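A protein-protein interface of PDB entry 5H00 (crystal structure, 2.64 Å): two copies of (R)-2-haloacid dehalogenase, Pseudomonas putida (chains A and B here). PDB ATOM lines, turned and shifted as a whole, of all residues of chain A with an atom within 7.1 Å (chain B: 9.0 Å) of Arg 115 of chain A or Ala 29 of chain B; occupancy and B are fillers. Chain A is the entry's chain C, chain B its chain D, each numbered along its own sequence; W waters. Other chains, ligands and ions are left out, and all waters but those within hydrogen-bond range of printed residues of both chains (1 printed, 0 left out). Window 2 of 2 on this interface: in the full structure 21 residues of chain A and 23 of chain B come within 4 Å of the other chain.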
ATOM      1  N   TYR A 112      13.465   1.458 -16.338  1.00  0.00           N
ATOM      2  CA  TYR A 112      12.353   1.285 -17.270  1.00  0.00           C
ATOM      3  C   TYR A 112      11.125   2.097 -16.898  1.00  0.00           C
ATOM      4  O   TYR A 112      10.675   2.036 -15.768  1.00  0.00           O
ATOM      5  CB  TYR A 112      11.968  -0.191 -17.360  1.00  0.00           C
ATOM      6  CG  TYR A 112      12.982  -1.060 -18.066  1.00  0.00           C
ATOM      7  CD1 TYR A 112      12.968  -1.200 -19.449  1.00  0.00           C
ATOM      8  CD2 TYR A 112      13.953  -1.747 -17.351  1.00  0.00           C
ATOM      9  CE1 TYR A 112      13.894  -2.000 -20.101  1.00  0.00           C
ATOM     10  CE2 TYR A 112      14.880  -2.544 -17.994  1.00  0.00           C
ATOM     11  CZ  TYR A 112      14.844  -2.664 -19.368  1.00  0.00           C
ATOM     12  OH  TYR A 112      15.770  -3.452 -19.996  1.00  0.00           O
ATOM     13  N   SER A 113      10.566   2.835 -17.851  1.00  0.00           N
ATOM     14  CA  SER A 113       9.381   3.632 -17.567  1.00  0.00           C
ATOM     15  C   SER A 113       8.145   2.751 -17.642  1.00  0.00           C
ATOM     16  O   SER A 113       8.230   1.630 -18.114  1.00  0.00           O
ATOM     17  CB  SER A 113       9.260   4.803 -18.529  1.00  0.00           C
ATOM     18  OG  SER A 113       8.799   4.378 -19.787  1.00  0.00           O
ATOM     19  N   VAL A 114       6.995   3.244 -17.191  1.00  0.00           N
ATOM     20  CA  VAL A 114       5.824   2.380 -17.137  1.00  0.00           C
ATOM     21  C   VAL A 114       5.360   1.992 -18.537  1.00  0.00           C
ATOM     22  O   VAL A 114       4.831   0.912 -18.731  1.00  0.00           O
ATOM     23  CB  VAL A 114       4.646   3.029 -16.358  1.00  0.00           C
ATOM     24  CG1 VAL A 114       5.029   3.256 -14.909  1.00  0.00           C
ATOM     25  CG2 VAL A 114       4.203   4.308 -17.001  1.00  0.00           C
ATOM     26  N   ARG A 115       5.583   2.857 -19.513  1.00  0.00           N
ATOM     27  CA  ARG A 115       5.205   2.541 -20.881  1.00  0.00           C
ATOM     28  C   ARG A 115       6.142   1.498 -21.469  1.00  0.00           C
ATOM     29  O   ARG A 115       5.723   0.673 -22.280  1.00  0.00           O
ATOM     30  CB  ARG A 115       5.182   3.801 -21.737  1.00  0.00           C
ATOM     31  CG  ARG A 115       4.178   4.787 -21.187  1.00  0.00           C
ATOM     32  CD  ARG A 115       3.910   5.988 -22.087  1.00  0.00           C
ATOM     33  NE  ARG A 115       3.814   7.264 -21.355  1.00  0.00           N
ATOM     34  CZ  ARG A 115       3.082   7.501 -20.257  1.00  0.00           C
ATOM     35  NH1 ARG A 115       2.311   6.567 -19.705  1.00  0.00           N
ATOM     36  NH2 ARG A 115       3.105   8.712 -19.709  1.00  0.00           N
ATOM     37  N   GLU A 116       7.402   1.517 -21.050  1.00  0.00           N
ATOM     38  CA  GLU A 116       8.322   0.471 -21.465  1.00  0.00           C
ATOM     39  C   GLU A 116       7.892  -0.898 -20.919  1.00  0.00           C
ATOM     40  O   GLU A 116       7.914  -1.893 -21.638  1.00  0.00           O
ATOM     41  CB  GLU A 116       9.744   0.804 -21.024  1.00  0.00           C
ATOM     42  CG  GLU A 116      10.312   2.011 -21.705  1.00  0.00           C
ATOM     43  CD  GLU A 116      11.787   2.180 -21.431  1.00  0.00           C
ATOM     44  OE1 GLU A 116      12.196   1.993 -20.272  1.00  0.00           O
ATOM     45  OE2 GLU A 116      12.545   2.484 -22.376  1.00  0.00           O
ATOM     46  N   ILE A 117       7.505  -0.941 -19.649  1.00  0.00           N
ATOM     47  CA  ILE A 117       7.030  -2.170 -19.044  1.00  0.00           C
ATOM     48  C   ILE A 117       5.765  -2.629 -19.759  1.00  0.00           C
ATOM     49  O   ILE A 117       5.489  -3.819 -19.857  1.00  0.00           O
ATOM     50  CB  ILE A 117       6.777  -1.995 -17.526  1.00  0.00           C
ATOM     51  CG1 ILE A 117       8.105  -1.943 -16.761  1.00  0.00           C
ATOM     52  CG2 ILE A 117       5.981  -3.152 -16.961  1.00  0.00           C
ATOM     53  CD1 ILE A 117       8.461  -0.617 -16.220  1.00  0.00           C
ATOM     54  N   GLY A 118       5.020  -1.685 -20.309  1.00  0.00           N
ATOM     55  CA  GLY A 118       3.800  -2.016 -21.014  1.00  0.00           C
ATOM     56  C   GLY A 118       4.085  -2.645 -22.356  1.00  0.00           C
ATOM     57  O   GLY A 118       3.441  -3.609 -22.763  1.00  0.00           O
ATOM     58  N   GLN A 119       5.065  -2.090 -23.047  1.00  0.00           N
ATOM     59  CA  GLN A 119       5.494  -2.630 -24.313  1.00  0.00           C
ATOM     60  C   GLN A 119       6.009  -4.042 -24.127  1.00  0.00           C
ATOM     61  O   GLN A 119       5.800  -4.898 -24.978  1.00  0.00           O
ATOM     62  CB  GLN A 119       6.563  -1.741 -24.934  1.00  0.00           C
ATOM     63  CG  GLN A 119       6.071  -0.358 -25.296  1.00  0.00           C
ATOM     64  CD  GLN A 119       7.181   0.532 -25.806  1.00  0.00           C
ATOM     65  OE1 GLN A 119       8.348   0.146 -25.809  1.00  0.00           O
ATOM     66  NE2 GLN A 119       6.823   1.735 -26.240  1.00  0.00           N
ATOM     67  N   ILE A 120       6.670  -4.288 -23.001  1.00  0.00           N
ATOM     68  CA  ILE A 120       7.162  -5.620 -22.701  1.00  0.00           C
ATOM     69  C   ILE A 120       6.020  -6.613 -22.532  1.00  0.00           C
ATOM     70  O   ILE A 120       6.072  -7.722 -23.057  1.00  0.00           O
ATOM     71  CB  ILE A 120       8.038  -5.613 -21.447  1.00  0.00           C
ATOM     72  CG1 ILE A 120       9.400  -5.022 -21.805  1.00  0.00           C
ATOM     73  CG2 ILE A 120       8.195  -7.026 -20.879  1.00  0.00           C
ATOM     74  CD1 ILE A 120      10.386  -5.036 -20.699  1.00  0.00           C
ATOM     75  N   ARG A 121       4.980  -6.208 -21.812  1.00  0.00           N
ATOM     76  CA  ARG A 121       3.831  -7.083 -21.589  1.00  0.00           C
ATOM     77  C   ARG A 121       3.163  -7.438 -22.896  1.00  0.00           C
ATOM     78  O   ARG A 121       2.726  -8.565 -23.080  1.00  0.00           O
ATOM     79  CB  ARG A 121       2.802  -6.437 -20.659  1.00  0.00           C
ATOM     80  CG  ARG A 121       3.291  -6.215 -19.267  1.00  0.00           C
ATOM     81  CD  ARG A 121       2.242  -5.551 -18.425  1.00  0.00           C
ATOM     82  NE  ARG A 121       2.604  -5.625 -17.019  1.00  0.00           N
ATOM     83  CZ  ARG A 121       2.899  -4.570 -16.285  1.00  0.00           C
ATOM     84  NH1 ARG A 121       2.835  -3.377 -16.839  1.00  0.00           N
ATOM     85  NH2 ARG A 121       3.232  -4.704 -15.011  1.00  0.00           N
ATOM     86  N   TRP A 212      15.114  -5.864 -25.274  1.00  0.00           N
ATOM     87  CA  TRP A 212      15.541  -5.261 -24.018  1.00  0.00           C
ATOM     88  C   TRP A 212      16.496  -6.200 -23.299  1.00  0.00           C
ATOM     89  O   TRP A 212      16.082  -6.906 -22.374  1.00  0.00           O
ATOM     90  CB  TRP A 212      14.347  -4.978 -23.097  1.00  0.00           C
ATOM     91  CG  TRP A 212      13.303  -4.116 -23.672  1.00  0.00           C
ATOM     92  CD1 TRP A 212      13.281  -2.767 -23.672  1.00  0.00           C
ATOM     93  CD2 TRP A 212      12.110  -4.539 -24.336  1.00  0.00           C
ATOM     94  NE1 TRP A 212      12.155  -2.308 -24.297  1.00  0.00           N
ATOM     95  CE2 TRP A 212      11.410  -3.381 -24.713  1.00  0.00           C
ATOM     96  CE3 TRP A 212      11.569  -5.790 -24.663  1.00  0.00           C
ATOM     97  CZ2 TRP A 212      10.194  -3.426 -25.392  1.00  0.00           C
ATOM     98  CZ3 TRP A 212      10.360  -5.835 -25.338  1.00  0.00           C
ATOM     99  CH2 TRP A 212       9.687  -4.660 -25.695  1.00  0.00           C
ATOM    100  N   PRO B  23      17.513  15.099 -20.070  1.00  0.00           N
ATOM    101  CA  PRO B  23      16.622  14.960 -21.221  1.00  0.00           C
ATOM    102  C   PRO B  23      15.369  14.164 -20.895  1.00  0.00           C
ATOM    103  O   PRO B  23      15.448  13.171 -20.196  1.00  0.00           O
ATOM    104  CB  PRO B  23      17.494  14.229 -22.241  1.00  0.00           C
ATOM    105  CG  PRO B  23      18.407  13.421 -21.425  1.00  0.00           C
ATOM    106  CD  PRO B  23      18.637  14.152 -20.132  1.00  0.00           C
ATOM    107  N   VAL B  24      14.230  14.617 -21.401  1.00  0.00           N
ATOM    108  CA  VAL B  24      12.959  13.936 -21.201  1.00  0.00           C
ATOM    109  C   VAL B  24      12.619  13.071 -22.413  1.00  0.00           C
ATOM    110  O   VAL B  24      12.200  13.586 -23.451  1.00  0.00           O
ATOM    111  CB  VAL B  24      11.811  14.946 -20.951  1.00  0.00           C
ATOM    112  CG1 VAL B  24      10.493  14.219 -20.694  1.00  0.00           C
ATOM    113  CG2 VAL B  24      12.160  15.870 -19.793  1.00  0.00           C
ATOM    114  N   PRO B  25      12.805  11.747 -22.278  1.00  0.00           N
ATOM    115  CA  PRO B  25      12.520  10.742 -23.306  1.00  0.00           C
ATOM    116  C   PRO B  25      11.065  10.789 -23.714  1.00  0.00           C
ATOM    117  O   PRO B  25      10.244  11.169 -22.903  1.00  0.00           O
ATOM    118  CB  PRO B  25      12.839   9.420 -22.611  1.00  0.00           C
ATOM    119  CG  PRO B  25      13.708   9.773 -21.476  1.00  0.00           C
ATOM    120  CD  PRO B  25      13.271  11.127 -21.029  1.00  0.00           C
ATOM    121  N   GLU B  26      10.746  10.410 -24.943  1.00  0.00           N
ATOM    122  CA  GLU B  26       9.354  10.397 -25.375  1.00  0.00           C
ATOM    123  C   GLU B  26       8.522   9.379 -24.598  1.00  0.00           C
ATOM    124  O   GLU B  26       7.315   9.541 -24.458  1.00  0.00           O
ATOM    125  CB  GLU B  26       9.241  10.097 -26.862  1.00  0.00           C
ATOM    126  CG  GLU B  26       9.795  11.152 -27.791  1.00  0.00           C
ATOM    127  CD  GLU B  26       9.471  10.838 -29.230  1.00  0.00           C
ATOM    128  OE1 GLU B  26      10.395  10.457 -29.976  1.00  0.00           O
ATOM    129  OE2 GLU B  26       8.291  10.978 -29.608  1.00  0.00           O
ATOM    130  N   HIS B  27       9.161   8.331 -24.092  1.00  0.00           N
ATOM    131  CA  HIS B  27       8.417   7.298 -23.389  1.00  0.00           C
ATOM    132  C   HIS B  27       8.151   7.714 -21.951  1.00  0.00           C
ATOM    133  O   HIS B  27       7.505   6.991 -21.208  1.00  0.00           O
ATOM    134  CB  HIS B  27       9.144   5.943 -23.438  1.00  0.00           C
ATOM    135  CG  HIS B  27      10.487   5.931 -22.778  1.00  0.00           C
ATOM    136  ND1 HIS B  27      10.652   5.696 -21.428  1.00  0.00           N
ATOM    137  CD2 HIS B  27      11.733   6.087 -23.283  1.00  0.00           C
ATOM    138  CE1 HIS B  27      11.937   5.728 -21.131  1.00  0.00           C
ATOM    139  NE2 HIS B  27      12.618   5.962 -22.241  1.00  0.00           N
ATOM    140  N   ARG B  28       8.633   8.893 -21.572  1.00  0.00           N
ATOM    141  CA  ARG B  28       8.365   9.437 -20.248  1.00  0.00           C
ATOM    142  C   ARG B  28       7.591  10.734 -20.298  1.00  0.00           C
ATOM    143  O   ARG B  28       6.962  11.111 -19.322  1.00  0.00           O
ATOM    144  CB  ARG B  28       9.658   9.676 -19.491  1.00  0.00           C
ATOM    145  CG  ARG B  28      10.333   8.434 -19.036  1.00  0.00           C
ATOM    146  CD  ARG B  28      11.578   8.776 -18.275  1.00  0.00           C
ATOM    147  NE  ARG B  28      12.386   7.588 -18.072  1.00  0.00           N
ATOM    148  CZ  ARG B  28      12.126   6.670 -17.153  1.00  0.00           C
ATOM    149  NH1 ARG B  28      11.082   6.816 -16.349  1.00  0.00           N
ATOM    150  NH2 ARG B  28      12.912   5.609 -17.042  1.00  0.00           N
ATOM    151  N   ALA B  29       7.649  11.413 -21.435  1.00  0.00           N
ATOM    152  CA  ALA B  29       7.049  12.732 -21.591  1.00  0.00           C
ATOM    153  C   ALA B  29       5.605  12.772 -21.113  1.00  0.00           C
ATOM    154  O   ALA B  29       4.835  11.854 -21.398  1.00  0.00           O
ATOM    155  CB  ALA B  29       7.127  13.167 -23.043  1.00  0.00           C
ATOM    156  N   ASP B  30       5.236  13.822 -20.378  1.00  0.00           N
ATOM    157  CA  ASP B  30       3.845  13.964 -19.946  1.00  0.00           C
ATOM    158  C   ASP B  30       3.023  14.383 -21.158  1.00  0.00           C
ATOM    159  O   ASP B  30       3.575  14.608 -22.231  1.00  0.00           O
ATOM    160  CB  ASP B  30       3.689  14.950 -18.773  1.00  0.00           C
ATOM    161  CG  ASP B  30       4.066  16.389 -19.123  1.00  0.00           C
ATOM    162  OD1 ASP B  30       4.031  16.788 -20.302  1.00  0.00           O
ATOM    163  OD2 ASP B  30       4.382  17.149 -18.187  1.00  0.00           O
ATOM    164  N   GLN B  31       1.715  14.499 -20.998  1.00  0.00           N
ATOM    165  CA  GLN B  31       0.855  14.673 -22.155  1.00  0.00           C
ATOM    166  C   GLN B  31       0.898  16.094 -22.703  1.00  0.00           C
ATOM    167  O   GLN B  31       0.627  16.303 -23.871  1.00  0.00           O
ATOM    168  CB  GLN B  31      -0.582  14.260 -21.806  1.00  0.00           C
ATOM    169  CG  GLN B  31      -1.074  12.989 -22.543  1.00  0.00           C
ATOM    170  CD  GLN B  31      -2.095  12.170 -21.738  1.00  0.00           C
ATOM    171  OE1 GLN B  31      -2.789  12.703 -20.883  1.00  0.00           O
ATOM    172  NE2 GLN B  31      -2.172  10.867 -22.005  1.00  0.00           N
ATOM    173  N   GLU B  32       1.252  17.065 -21.872  1.00  0.00           N
ATOM    174  CA  GLU B  32       1.418  18.442 -22.350  1.00  0.00           C
ATOM    175  C   GLU B  32       2.680  18.584 -23.199  1.00  0.00           C
ATOM    176  O   GLU B  32       2.671  19.220 -24.247  1.00  0.00           O
ATOM    177  CB  GLU B  32       1.478  19.447 -21.186  1.00  0.00           C
ATOM    178  CG  GLU B  32       1.723  20.890 -21.653  1.00  0.00           C
ATOM    179  CD  GLU B  32       2.339  21.788 -20.597  1.00  0.00           C
ATOM    180  OE1 GLU B  32       1.684  22.048 -19.570  1.00  0.00           O
ATOM    181  OE2 GLU B  32       3.480  22.246 -20.800  1.00  0.00           O
ATOM    182  N   LEU B  33       3.769  17.997 -22.722  1.00  0.00           N
ATOM    183  CA  LEU B  33       5.026  18.019 -23.452  1.00  0.00           C
ATOM    184  C   LEU B  33       4.923  17.168 -24.721  1.00  0.00           C
ATOM    185  O   LEU B  33       5.365  17.582 -25.788  1.00  0.00           O
ATOM    186  CB  LEU B  33       6.175  17.534 -22.561  1.00  0.00           C
ATOM    187  CG  LEU B  33       7.583  17.512 -23.162  1.00  0.00           C
ATOM    188  CD1 LEU B  33       7.954  18.876 -23.751  1.00  0.00           C
ATOM    189  CD2 LEU B  33       8.619  17.055 -22.134  1.00  0.00           C
ATOM    190  N   SER B  34       4.309  15.995 -24.602  1.00  0.00           N
ATOM    191  CA  SER B  34       4.076  15.111 -25.741  1.00  0.00           C
ATOM    192  C   SER B  34       3.364  15.802 -26.909  1.00  0.00           C
ATOM    193  O   SER B  34       3.483  15.375 -28.049  1.00  0.00           O
ATOM    194  CB  SER B  34       3.269  13.884 -25.300  1.00  0.00           C
ATOM    195  OG  SER B  34       4.043  13.003 -24.504  1.00  0.00           O
ATOM    196  N   GLU B  35       2.635  16.872 -26.624  1.00  0.00           N
ATOM    197  CA  GLU B  35       1.949  17.606 -27.672  1.00  0.00           C
ATOM    198  C   GLU B  35       2.924  18.479 -28.430  1.00  0.00           C
ATOM    199  O   GLU B  35       2.869  18.564 -29.653  1.00  0.00           O
ATOM    200  CB  GLU B  35       0.820  18.456 -27.094  1.00  0.00           C
ATOM    201  CG  GLU B  35      -0.237  18.839 -28.115  1.00  0.00           C
ATOM    202  CD  GLU B  35      -0.323  20.339 -28.353  1.00  0.00           C
ATOM    203  OE1 GLU B  35       0.404  21.102 -27.676  1.00  0.00           O
ATOM    204  OE2 GLU B  35      -1.130  20.758 -29.212  1.00  0.00           O
ATOM    205  N   ILE B  36       3.813  19.140 -27.702  1.00  0.00           N
ATOM    206  CA  ILE B  36       4.876  19.899 -28.342  1.00  0.00           C
ATOM    207  C   ILE B  36       5.712  18.954 -29.196  1.00  0.00           C
ATOM    208  O   ILE B  36       5.927  19.203 -30.369  1.00  0.00           O
ATOM    209  CB  ILE B  36       5.779  20.595 -27.323  1.00  0.00           C
ATOM    210  CG1 ILE B  36       4.961  21.476 -26.380  1.00  0.00           C
ATOM    211  CG2 ILE B  36       6.830  21.418 -28.032  1.00  0.00           C
ATOM    212  CD1 ILE B  36       5.732  21.889 -25.140  1.00  0.00           C
ATOM    213  N   TYR B  37       6.157  17.864 -28.582  1.00  0.00           N
ATOM    214  CA  TYR B  37       6.940  16.846 -29.255  1.00  0.00           C
ATOM    215  C   TYR B  37       6.311  16.452 -30.568  1.00  0.00           C
ATOM    216  O   TYR B  37       6.986  16.368 -31.587  1.00  0.00           O
ATOM    217  CB  TYR B  37       7.097  15.610 -28.367  1.00  0.00           C
ATOM    218  CG  TYR B  37       8.192  15.733 -27.337  1.00  0.00           C
ATOM    219  CD1 TYR B  37       8.879  16.925 -27.166  1.00  0.00           C
ATOM    220  CD2 TYR B  37       8.545  14.656 -26.538  1.00  0.00           C
ATOM    221  CE1 TYR B  37       9.879  17.045 -26.223  1.00  0.00           C
ATOM    222  CE2 TYR B  37       9.551  14.769 -25.594  1.00  0.00           C
ATOM    223  CZ  TYR B  37      10.212  15.966 -25.447  1.00  0.00           C
ATOM    224  OH  TYR B  37      11.209  16.096 -24.518  1.00  0.00           O
ATOM    225  N   ARG B  38       5.008  16.222 -30.542  1.00  0.00           N
ATOM    226  CA  ARG B  38       4.317  15.813 -31.738  1.00  0.00           C
ATOM    227  C   ARG B  38       4.345  16.919 -32.800  1.00  0.00           C
ATOM    228  O   ARG B  38       4.436  16.627 -33.987  1.00  0.00           O
ATOM    229  CB  ARG B  38       2.879  15.398 -31.410  1.00  0.00           C
ATOM    230  CG  ARG B  38       2.279  14.437 -32.430  1.00  0.00           C
ATOM    231  CD  ARG B  38       2.262  12.983 -31.944  1.00  0.00           C
ATOM    232  NE  ARG B  38       1.733  12.051 -32.951  1.00  0.00           N
ATOM    233  CZ  ARG B  38       2.470  11.320 -33.790  1.00  0.00           C
ATOM    234  NH1 ARG B  38       3.793  11.346 -33.728  1.00  0.00           N
ATOM    235  NH2 ARG B  38       1.876  10.528 -34.672  1.00  0.00           N
ATOM    236  N   VAL B  49      12.157  12.426 -31.608  1.00  0.00           N
ATOM    237  CA  VAL B  49      12.468  13.697 -30.976  1.00  0.00           C
ATOM    238  C   VAL B  49      13.911  13.608 -30.532  1.00  0.00           C
ATOM    239  O   VAL B  49      14.282  12.694 -29.794  1.00  0.00           O
ATOM    240  CB  VAL B  49      11.545  13.996 -29.779  1.00  0.00           C
ATOM    241  CG1 VAL B  49      11.971  15.263 -29.065  1.00  0.00           C
ATOM    242  CG2 VAL B  49      10.102  14.090 -30.234  1.00  0.00           C
ATOM    243  N   GLN B  54      15.111  16.998 -26.317  1.00  0.00           N
ATOM    244  CA  GLN B  54      14.760  16.356 -25.056  1.00  0.00           C
ATOM    245  C   GLN B  54      15.346  17.148 -23.896  1.00  0.00           C
ATOM    246  O   GLN B  54      14.684  17.392 -22.897  1.00  0.00           O
ATOM    247  CB  GLN B  54      15.261  14.905 -25.012  1.00  0.00           C
ATOM    248  CG  GLN B  54      14.519  13.949 -25.916  1.00  0.00           C
ATOM    249  CD  GLN B  54      15.220  12.603 -26.068  1.00  0.00           C
ATOM    250  OE1 GLN B  54      15.612  11.970 -25.087  1.00  0.00           O
ATOM    251  NE2 GLN B  54      15.387  12.168 -27.306  1.00  0.00           N
ATOM    252  N   ALA B  57      13.816  20.598 -23.440  1.00  0.00           N
ATOM    253  CA  ALA B  57      12.466  20.493 -22.887  1.00  0.00           C
ATOM    254  C   ALA B  57      12.449  20.592 -21.363  1.00  0.00           C
ATOM    255  O   ALA B  57      11.433  20.944 -20.765  1.00  0.00           O
ATOM    256  CB  ALA B  57      11.835  19.213 -23.311  1.00  0.00           C
ATOM    257  N   ARG B  60      11.338  23.833 -19.706  1.00  0.00           N
ATOM    258  CA  ARG B  60      10.101  23.808 -20.468  1.00  0.00           C
ATOM    259  C   ARG B  60       9.533  25.146 -20.940  1.00  0.00           C
ATOM    260  O   ARG B  60       9.090  25.226 -22.086  1.00  0.00           O
ATOM    261  CB  ARG B  60       9.043  23.078 -19.666  1.00  0.00           C
ATOM    262  CG  ARG B  60       7.944  22.516 -20.510  1.00  0.00           C
ATOM    263  CD  ARG B  60       7.675  21.098 -20.086  1.00  0.00           C
ATOM    264  NE  ARG B  60       6.265  20.756 -20.198  1.00  0.00           N
ATOM    265  CZ  ARG B  60       5.707  19.720 -19.588  1.00  0.00           C
ATOM    266  NH1 ARG B  60       6.441  18.924 -18.824  1.00  0.00           N
ATOM    267  NH2 ARG B  60       4.415  19.484 -19.742  1.00  0.00           N
ATOM    268  N   ILE B 173       8.119   5.561 -33.856  1.00  0.00           N
ATOM    269  CA  ILE B 173       9.361   5.984 -33.234  1.00  0.00           C
ATOM    270  C   ILE B 173      10.365   4.889 -33.549  1.00  0.00           C
ATOM    271  O   ILE B 173      10.032   3.715 -33.477  1.00  0.00           O
ATOM    272  CB  ILE B 173       9.208   6.187 -31.707  1.00  0.00           C
ATOM    273  CG1 ILE B 173       8.114   7.209 -31.407  1.00  0.00           C
ATOM    274  CG2 ILE B 173      10.496   6.669 -31.077  1.00  0.00           C
ATOM    275  CD1 ILE B 173       7.737   7.297 -29.913  1.00  0.00           C
ATOM    276  N   HIS B 180      19.668   1.783 -20.244  1.00  0.00           N
ATOM    277  CA  HIS B 180      19.192   0.818 -19.258  1.00  0.00           C
ATOM    278  C   HIS B 180      18.672  -0.484 -19.898  1.00  0.00           C
ATOM    279  O   HIS B 180      18.511  -1.493 -19.213  1.00  0.00           O
ATOM    280  CB  HIS B 180      18.120   1.443 -18.342  1.00  0.00           C
ATOM    281  CG  HIS B 180      16.914   1.957 -19.055  1.00  0.00           C
ATOM    282  ND1 HIS B 180      16.933   3.098 -19.824  1.00  0.00           N
ATOM    283  CD2 HIS B 180      15.640   1.507 -19.084  1.00  0.00           C
ATOM    284  CE1 HIS B 180      15.725   3.323 -20.305  1.00  0.00           C
ATOM    285  NE2 HIS B 180      14.922   2.374 -19.872  1.00  0.00           N
ATOM    286  N   HIS B 181      18.420  -0.480 -21.202  1.00  0.00           N
ATOM    287  CA  HIS B 181      18.110  -1.738 -21.873  1.00  0.00           C
ATOM    288  C   HIS B 181      19.398  -2.534 -21.980  1.00  0.00           C
ATOM    289  O   HIS B 181      19.417  -3.739 -21.733  1.00  0.00           O
ATOM    290  CB  HIS B 181      17.506  -1.531 -23.266  1.00  0.00           C
ATOM    291  CG  HIS B 181      16.318  -0.632 -23.291  1.00  0.00           C
ATOM    292  ND1 HIS B 181      15.781  -0.138 -24.460  1.00  0.00           N
ATOM    293  CD2 HIS B 181      15.554  -0.120 -22.294  1.00  0.00           C
ATOM    294  CE1 HIS B 181      14.750   0.634 -24.189  1.00  0.00           C
ATOM    295  NE2 HIS B 181      14.589   0.658 -22.872  1.00  0.00           N
HETATM  296  O   HOH W   1       6.034   6.095 -18.764  1.00  0.00           O
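O of His 180 of chain B lies within hydrogen-bond range of OH of Tyr 112 of chain A (3.5 Å).
The side-chain hydroxyl (OG) of Ser 113 of chain A sits at hydrogen-bond distance from a ring nitrogen (ND1) of His 27 of chain B (2.8 Å).
The side-chain carboxylate (OE2) of Glu 116 of chain A is in hydrogen-bond range of a ring nitrogen (NE2) of His 27 of chain B, 3.5 Å away.
A ring nitrogen (NE2) of His 180 of chain B sits at hydrogen-bond distance from the side-chain carboxylate (OE1) of Glu 116 of chain A (2.8 Å).
The side-chain carboxylate (OE2) of Glu 116 of chain A is in hydrogen-bond range of a ring nitrogen (NE2) of His 181 of chain B.
The side-chain carboxylate (OE1) of Glu 116 of chain A sits at hydrogen-bond distance from the backbone NH (N) of Ser 113 of chain A (3.0 Å).
OG of Ser 34 of chain B is in hydrogen-bond range of O of Ala 29 of chain B (3.4 Å).
A ring nitrogen (NE2) of His 181 of chain B lies within hydrogen-bond range of a ring nitrogen (NE2) of His 180 of chain B, at 3.5 Å.
Among the printed residues, pairs that only touch across the chains: Tyr 112 of chain A with Arg 28 of chain B, Tyr 112 of chain A with His 181 of chain B, Ser 113 of chain A with Arg 28 of chain B, Arg 115 of chain A with His 27 of chain B, Arg 115 of chain A with Ala 29 of chain B and Trp 212 of chain A with His 181 of chain B.
Of the printed residues of chain B, Ser 113 of chain A touches His 27 (2.8 Å) and Arg 28 (3.5 Å).
Arg 115 of chain A touches two residues of chain B.
No residue of chain B comes within 4 Å of Gly 118 of chain A.
Printed residues of chain A within 4 Å of His 27 of chain B: Ser 113, Arg 115 and Glu 116.
Printed residues of chain A within 4 Å of Arg 28 of chain B: Tyr 112 and Ser 113.
Of chain A, only Arg 115 comes within 4 Å of Ala 29 of chain B.
Printed residues of chain A within 4 Å of His 180 of chain B: Tyr 112 and Glu 116.
Of the printed residues of chain A, His 181 of chain B touches Tyr 112, Glu 116 and Trp 212.
The nearest residue of chain B that does not touch Arg 115 of chain A is Arg 28 of chain B (4.6 Å).
Of the 11 printed residues of chain A, 5 touch a printed residue of chain B.
Along chain A the printed residues that touch a printed residue of chain B span positions 112 to 212.
Among the printed residues, 11 pairs touch across the chains.
No position is printed for both chains.
Of the 11 pairs that touch across the chains among the printed residues, none has its exchanged pair printed and touching as well.
Water W1 lies within hydrogen-bond range of O of His 27 of chain B (3.0 Å), N of Arg 115 of chain A (3.4 Å), N of Val 114 of chain A (3.4 Å) and OG of Ser 113 of chain A (3.4 Å).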
